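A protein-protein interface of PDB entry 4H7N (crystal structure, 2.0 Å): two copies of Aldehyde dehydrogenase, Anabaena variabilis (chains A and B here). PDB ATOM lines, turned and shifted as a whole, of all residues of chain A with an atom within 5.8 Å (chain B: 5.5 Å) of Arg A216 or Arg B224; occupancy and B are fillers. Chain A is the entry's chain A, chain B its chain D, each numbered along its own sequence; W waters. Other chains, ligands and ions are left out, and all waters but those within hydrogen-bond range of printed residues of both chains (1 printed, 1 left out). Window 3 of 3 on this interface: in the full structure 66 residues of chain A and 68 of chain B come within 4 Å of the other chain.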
ATOM      1  N   SER A 211     -15.618   3.875 -18.089  1.00  0.00           N
ATOM      2  CA  SER A 211     -15.752   2.516 -18.540  1.00  0.00           C
ATOM      3  C   SER A 211     -14.391   1.792 -18.628  1.00  0.00           C
ATOM      4  O   SER A 211     -13.369   2.418 -18.859  1.00  0.00           O
ATOM      5  CB  SER A 211     -16.406   2.512 -19.922  1.00  0.00           C
ATOM      6  OG  SER A 211     -15.435   2.718 -20.939  1.00  0.00           O
ATOM      7  N   VAL A 212     -14.413   0.471 -18.519  1.00  0.00           N
ATOM      8  CA  VAL A 212     -13.183  -0.307 -18.579  1.00  0.00           C
ATOM      9  C   VAL A 212     -12.500  -0.142 -19.919  1.00  0.00           C
ATOM     10  O   VAL A 212     -11.269  -0.010 -19.972  1.00  0.00           O
ATOM     11  CB  VAL A 212     -13.423  -1.811 -18.312  1.00  0.00           C
ATOM     12  CG1 VAL A 212     -12.125  -2.596 -18.423  1.00  0.00           C
ATOM     13  CG2 VAL A 212     -13.891  -1.984 -16.898  1.00  0.00           C
ATOM     14  N   ALA A 213     -13.243  -0.155 -21.021  1.00  0.00           N
ATOM     15  CA  ALA A 213     -12.564  -0.054 -22.312  1.00  0.00           C
ATOM     16  C   ALA A 213     -11.875   1.330 -22.503  1.00  0.00           C
ATOM     17  O   ALA A 213     -10.792   1.435 -23.078  1.00  0.00           O
ATOM     18  CB  ALA A 213     -13.527  -0.367 -23.456  1.00  0.00           C
ATOM     19  N   THR A 214     -12.499   2.403 -22.058  1.00  0.00           N
ATOM     20  CA  THR A 214     -11.888   3.726 -22.243  1.00  0.00           C
ATOM     21  C   THR A 214     -10.707   3.871 -21.254  1.00  0.00           C
ATOM     22  O   THR A 214      -9.678   4.448 -21.571  1.00  0.00           O
ATOM     23  CB  THR A 214     -12.907   4.825 -21.969  1.00  0.00           C
ATOM     24  OG1 THR A 214     -14.039   4.615 -22.820  1.00  0.00           O
ATOM     25  CG2 THR A 214     -12.295   6.211 -22.219  1.00  0.00           C
ATOM     26  N   GLY A 215     -10.856   3.295 -20.084  1.00  0.00           N
ATOM     27  CA  GLY A 215      -9.823   3.381 -19.048  1.00  0.00           C
ATOM     28  C   GLY A 215      -8.569   2.636 -19.460  1.00  0.00           C
ATOM     29  O   GLY A 215      -7.449   3.068 -19.155  1.00  0.00           O
ATOM     30  N   ARG A 216      -8.762   1.524 -20.145  1.00  0.00           N
ATOM     31  CA  ARG A 216      -7.645   0.777 -20.672  1.00  0.00           C
ATOM     32  C   ARG A 216      -6.876   1.621 -21.700  1.00  0.00           C
ATOM     33  O   ARG A 216      -5.645   1.614 -21.734  1.00  0.00           O
ATOM     34  CB  ARG A 216      -8.082  -0.548 -21.255  1.00  0.00           C
ATOM     35  CG  ARG A 216      -8.475  -1.505 -20.177  1.00  0.00           C
ATOM     36  CD  ARG A 216      -8.628  -2.879 -20.673  1.00  0.00           C
ATOM     37  NE  ARG A 216      -7.338  -3.512 -20.917  1.00  0.00           N
ATOM     38  CZ  ARG A 216      -7.206  -4.776 -21.301  1.00  0.00           C
ATOM     39  NH1 ARG A 216      -8.280  -5.519 -21.479  1.00  0.00           N
ATOM     40  NH2 ARG A 216      -6.012  -5.322 -21.508  1.00  0.00           N
ATOM     41  N   GLU A 217      -7.605   2.383 -22.500  1.00  0.00           N
ATOM     42  CA  GLU A 217      -6.987   3.240 -23.483  1.00  0.00           C
ATOM     43  C   GLU A 217      -6.254   4.382 -22.763  1.00  0.00           C
ATOM     44  O   GLU A 217      -5.164   4.779 -23.158  1.00  0.00           O
ATOM     45  CB  GLU A 217      -8.124   3.713 -24.379  1.00  0.00           C
ATOM     46  CG  GLU A 217      -7.840   4.662 -25.510  1.00  0.00           C
ATOM     47  CD  GLU A 217      -9.124   4.866 -26.354  1.00  0.00           C
ATOM     48  OE1 GLU A 217     -10.121   4.128 -26.139  1.00  0.00           O
ATOM     49  OE2 GLU A 217      -9.134   5.766 -27.223  1.00  0.00           O
ATOM     50  N   VAL A 218      -6.827   4.899 -21.677  1.00  0.00           N
ATOM     51  CA  VAL A 218      -6.162   5.968 -20.918  1.00  0.00           C
ATOM     52  C   VAL A 218      -4.888   5.448 -20.254  1.00  0.00           C
ATOM     53  O   VAL A 218      -3.915   6.147 -20.201  1.00  0.00           O
ATOM     54  CB  VAL A 218      -7.071   6.579 -19.830  1.00  0.00           C
ATOM     55  CG1 VAL A 218      -6.251   7.475 -18.893  1.00  0.00           C
ATOM     56  CG2 VAL A 218      -8.171   7.382 -20.476  1.00  0.00           C
ATOM     57  N   ALA A 219      -4.912   4.218 -19.749  1.00  0.00           N
ATOM     58  CA  ALA A 219      -3.706   3.558 -19.181  1.00  0.00           C
ATOM     59  C   ALA A 219      -2.605   3.528 -20.197  1.00  0.00           C
ATOM     60  O   ALA A 219      -1.420   3.831 -19.918  1.00  0.00           O
ATOM     61  CB  ALA A 219      -4.029   2.116 -18.749  1.00  0.00           C
ATOM     62  N   GLU A 220      -2.964   3.085 -21.386  1.00  0.00           N
ATOM     63  CA  GLU A 220      -1.955   2.916 -22.436  1.00  0.00           C
ATOM     64  C   GLU A 220      -1.424   4.257 -22.913  1.00  0.00           C
ATOM     65  O   GLU A 220      -0.262   4.396 -23.049  1.00  0.00           O
ATOM     66  CB  GLU A 220      -2.505   2.076 -23.614  1.00  0.00           C
ATOM     67  CG  GLU A 220      -2.800   0.618 -23.229  1.00  0.00           C
ATOM     68  CD  GLU A 220      -3.612  -0.163 -24.271  1.00  0.00           C
ATOM     69  OE1 GLU A 220      -3.427   0.109 -25.476  1.00  0.00           O
ATOM     70  OE2 GLU A 220      -4.414  -1.066 -23.876  1.00  0.00           O
ATOM     71  N   THR A 221      -2.277   5.266 -23.081  1.00  0.00           N
ATOM     72  CA  THR A 221      -1.831   6.628 -23.426  1.00  0.00           C
ATOM     73  C   THR A 221      -0.952   7.247 -22.362  1.00  0.00           C
ATOM     74  O   THR A 221       0.115   7.807 -22.641  1.00  0.00           O
ATOM     75  CB  THR A 221      -3.036   7.539 -23.702  1.00  0.00           C
ATOM     76  OG1 THR A 221      -3.812   6.952 -24.729  1.00  0.00           O
ATOM     77  CG2 THR A 221      -2.595   8.894 -24.195  1.00  0.00           C
ATOM     78  N   ARG A 224       2.538   5.737 -22.558  1.00  0.00           N
ATOM     79  CA  ARG A 224       3.320   6.244 -23.675  1.00  0.00           C
ATOM     80  C   ARG A 224       3.810   7.648 -23.421  1.00  0.00           C
ATOM     81  O   ARG A 224       4.889   8.002 -23.850  1.00  0.00           O
ATOM     82  CB  ARG A 224       2.496   6.295 -24.950  1.00  0.00           C
ATOM     83  CG  ARG A 224       2.312   4.959 -25.614  1.00  0.00           C
ATOM     84  CD  ARG A 224       1.788   5.128 -27.055  1.00  0.00           C
ATOM     85  NE  ARG A 224       0.360   5.397 -27.021  1.00  0.00           N
ATOM     86  CZ  ARG A 224      -0.565   4.449 -26.853  1.00  0.00           C
ATOM     87  NH1 ARG A 224      -0.196   3.167 -26.721  1.00  0.00           N
ATOM     88  NH2 ARG A 224      -1.857   4.773 -26.836  1.00  0.00           N
ATOM     89  N   LEU A 231      -6.834   5.353 -12.129  1.00  0.00           N
ATOM     90  CA  LEU A 231      -7.951   4.848 -12.899  1.00  0.00           C
ATOM     91  C   LEU A 231      -8.990   4.146 -12.011  1.00  0.00           C
ATOM     92  O   LEU A 231      -8.655   3.219 -11.244  1.00  0.00           O
ATOM     93  CB  LEU A 231      -7.487   3.822 -13.929  1.00  0.00           C
ATOM     94  CG  LEU A 231      -6.324   4.231 -14.796  1.00  0.00           C
ATOM     95  CD1 LEU A 231      -5.864   3.021 -15.568  1.00  0.00           C
ATOM     96  CD2 LEU A 231      -6.726   5.334 -15.733  1.00  0.00           C
ATOM     97  N   LEU A 233     -12.551   2.216 -12.871  1.00  0.00           N
ATOM     98  CA  LEU A 233     -13.163   1.787 -14.140  1.00  0.00           C
ATOM     99  C   LEU A 233     -14.434   0.959 -14.002  1.00  0.00           C
ATOM    100  O   LEU A 233     -14.795   0.204 -14.885  1.00  0.00           O
ATOM    101  CB  LEU A 233     -12.174   0.991 -14.976  1.00  0.00           C
ATOM    102  CG  LEU A 233     -10.819   1.639 -15.230  1.00  0.00           C
ATOM    103  CD1 LEU A 233     -10.049   0.845 -16.261  1.00  0.00           C
ATOM    104  CD2 LEU A 233     -11.030   3.097 -15.666  1.00  0.00           C
ATOM    105  N   PHE A 437      -9.948  -5.603 -13.208  1.00  0.00           N
ATOM    106  CA  PHE A 437      -9.979  -4.469 -14.153  1.00  0.00           C
ATOM    107  C   PHE A 437     -10.691  -3.235 -13.640  1.00  0.00           C
ATOM    108  O   PHE A 437     -10.930  -2.325 -14.406  1.00  0.00           O
ATOM    109  CB  PHE A 437     -10.590  -4.882 -15.515  1.00  0.00           C
ATOM    110  CG  PHE A 437      -9.665  -5.726 -16.342  1.00  0.00           C
ATOM    111  CD1 PHE A 437      -8.668  -5.133 -17.107  1.00  0.00           C
ATOM    112  CD2 PHE A 437      -9.721  -7.109 -16.285  1.00  0.00           C
ATOM    113  CE1 PHE A 437      -7.775  -5.913 -17.846  1.00  0.00           C
ATOM    114  CE2 PHE A 437      -8.846  -7.905 -17.043  1.00  0.00           C
ATOM    115  CZ  PHE A 437      -7.865  -7.299 -17.816  1.00  0.00           C
ATOM    116  N   ALA B 219       6.811  -0.062 -19.548  1.00  0.00           N
ATOM    117  CA  ALA B 219       5.639   0.730 -19.131  1.00  0.00           C
ATOM    118  C   ALA B 219       4.472   0.513 -20.032  1.00  0.00           C
ATOM    119  O   ALA B 219       3.300   0.379 -19.568  1.00  0.00           O
ATOM    120  CB  ALA B 219       5.945   2.223 -19.086  1.00  0.00           C
ATOM    121  N   GLU B 220       4.739   0.567 -21.329  1.00  0.00           N
ATOM    122  CA  GLU B 220       3.660   0.420 -22.304  1.00  0.00           C
ATOM    123  C   GLU B 220       3.089  -0.999 -22.300  1.00  0.00           C
ATOM    124  O   GLU B 220       1.878  -1.197 -22.359  1.00  0.00           O
ATOM    125  CB  GLU B 220       4.140   0.900 -23.696  1.00  0.00           C
ATOM    126  CG  GLU B 220       4.424   2.413 -23.692  1.00  0.00           C
ATOM    127  CD  GLU B 220       5.216   2.903 -24.919  1.00  0.00           C
ATOM    128  OE1 GLU B 220       4.989   2.347 -26.007  1.00  0.00           O
ATOM    129  OE2 GLU B 220       6.039   3.851 -24.803  1.00  0.00           O
ATOM    130  N   THR B 221       3.943  -2.008 -22.179  1.00  0.00           N
ATOM    131  CA  THR B 221       3.477  -3.404 -22.054  1.00  0.00           C
ATOM    132  C   THR B 221       2.687  -3.687 -20.786  1.00  0.00           C
ATOM    133  O   THR B 221       1.661  -4.381 -20.814  1.00  0.00           O
ATOM    134  CB  THR B 221       4.669  -4.337 -22.134  1.00  0.00           C
ATOM    135  OG1 THR B 221       5.364  -3.997 -23.315  1.00  0.00           O
ATOM    136  CG2 THR B 221       4.256  -5.795 -22.159  1.00  0.00           C
ATOM    137  N   ALA B 222       3.167  -3.186 -19.655  1.00  0.00           N
ATOM    138  CA  ALA B 222       2.444  -3.318 -18.379  1.00  0.00           C
ATOM    139  C   ALA B 222       1.040  -2.693 -18.452  1.00  0.00           C
ATOM    140  O   ALA B 222       0.079  -3.293 -17.981  1.00  0.00           O
ATOM    141  CB  ALA B 222       3.230  -2.677 -17.261  1.00  0.00           C
ATOM    142  N   ALA B 223       0.950  -1.497 -19.003  1.00  0.00           N
ATOM    143  CA  ALA B 223      -0.328  -0.837 -19.195  1.00  0.00           C
ATOM    144  C   ALA B 223      -1.306  -1.615 -20.137  1.00  0.00           C
ATOM    145  O   ALA B 223      -2.463  -1.785 -19.815  1.00  0.00           O
ATOM    146  CB  ALA B 223      -0.105   0.576 -19.664  1.00  0.00           C
ATOM    147  N   ARG B 224      -0.794  -2.198 -21.194  1.00  0.00           N
ATOM    148  CA  ARG B 224      -1.613  -3.033 -22.074  1.00  0.00           C
ATOM    149  C   ARG B 224      -2.040  -4.318 -21.361  1.00  0.00           C
ATOM    150  O   ARG B 224      -3.181  -4.767 -21.547  1.00  0.00           O
ATOM    151  CB  ARG B 224      -0.823  -3.235 -23.379  1.00  0.00           C
ATOM    152  CG  ARG B 224      -1.330  -4.212 -24.405  1.00  0.00           C
ATOM    153  CD  ARG B 224      -0.288  -4.321 -25.556  1.00  0.00           C
ATOM    154  NE  ARG B 224       0.373  -3.026 -25.862  1.00  0.00           N
ATOM    155  CZ  ARG B 224       1.691  -2.774 -25.816  1.00  0.00           C
ATOM    156  NH1 ARG B 224       2.570  -3.707 -25.492  1.00  0.00           N
ATOM    157  NH2 ARG B 224       2.147  -1.566 -26.121  1.00  0.00           N
ATOM    158  N   ARG B 225      -1.204  -4.887 -20.462  1.00  0.00           N
ATOM    159  CA  ARG B 225      -1.669  -6.013 -19.676  1.00  0.00           C
ATOM    160  C   ARG B 225      -2.566  -5.567 -18.505  1.00  0.00           C
ATOM    161  O   ARG B 225      -3.191  -6.378 -17.871  1.00  0.00           O
ATOM    162  CB  ARG B 225      -0.496  -6.812 -19.131  1.00  0.00           C
ATOM    163  CG  ARG B 225       0.335  -7.370 -20.275  1.00  0.00           C
ATOM    164  CD  ARG B 225       0.707  -8.801 -20.049  1.00  0.00           C
ATOM    165  NE  ARG B 225      -0.396  -9.615 -19.553  1.00  0.00           N
ATOM    166  CZ  ARG B 225      -0.503 -10.108 -18.303  1.00  0.00           C
ATOM    167  NH1 ARG B 225      -1.593 -10.837 -18.028  1.00  0.00           N
ATOM    168  NH2 ARG B 225       0.453  -9.906 -17.330  1.00  0.00           N
ATOM    169  N   PHE B 226      -2.545  -4.285 -18.179  1.00  0.00           N
ATOM    170  CA  PHE B 226      -3.250  -3.774 -17.043  1.00  0.00           C
ATOM    171  C   PHE B 226      -2.700  -4.295 -15.714  1.00  0.00           C
ATOM    172  O   PHE B 226      -3.452  -4.735 -14.831  1.00  0.00           O
ATOM    173  CB  PHE B 226      -4.803  -3.958 -17.181  1.00  0.00           C
ATOM    174  CG  PHE B 226      -5.616  -2.913 -16.447  1.00  0.00           C
ATOM    175  CD1 PHE B 226      -5.747  -1.666 -16.950  1.00  0.00           C
ATOM    176  CD2 PHE B 226      -6.217  -3.201 -15.240  1.00  0.00           C
ATOM    177  CE1 PHE B 226      -6.496  -0.680 -16.307  1.00  0.00           C
ATOM    178  CE2 PHE B 226      -6.976  -2.227 -14.571  1.00  0.00           C
ATOM    179  CZ  PHE B 226      -7.134  -0.973 -15.121  1.00  0.00           C
HETATM  180  O   HOH W   1       6.612   5.490 -22.537  1.00  0.00           O
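Of the printed residues of chain B, Ala A219 touches Ala B223 (3.5 Å).
Of the printed residues of chain B, Arg A224 touches Glu B220 (3.6 Å).
Of the printed residues of chain B, Leu A231 touches Phe B226.
Of the printed residues of chain A, Glu B220 touches Arg A224 (3.6 Å).
Water W1 lies within hydrogen-bond range of the side-chain carboxylate (OE2) of Glu B220 and the backbone carbonyl oxygen (O) of Arg A224.
Among the printed residues, merely in contact across the chains: Ala A219 with Ala B223, Glu A220 with Arg B224, Arg A224 with Glu B220, Leu A231 with Phe B226, Leu A233 with Phe B226 and Phe A437 with Phe B226.
Hydrophobic or aromatic side chains of chain B within 4 Å of the printed part of chain A: Ala B223 and Phe B226.
Hydrophobic or aromatic side chains of chain A within 4 Å of the printed part of chain B: Leu A231, Leu A233 and Phe A437.
Glu A220 touches Arg B224, and with the chains exchanged Arg A224 touches Glu B220.
Of the 7 pairs that touch across the chains among the printed residues, 2 have their exchanged pair printed and touching as well.
O of Arg B224 lies within hydrogen-bond range of NH2 of Arg A216 (2.9 Å).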
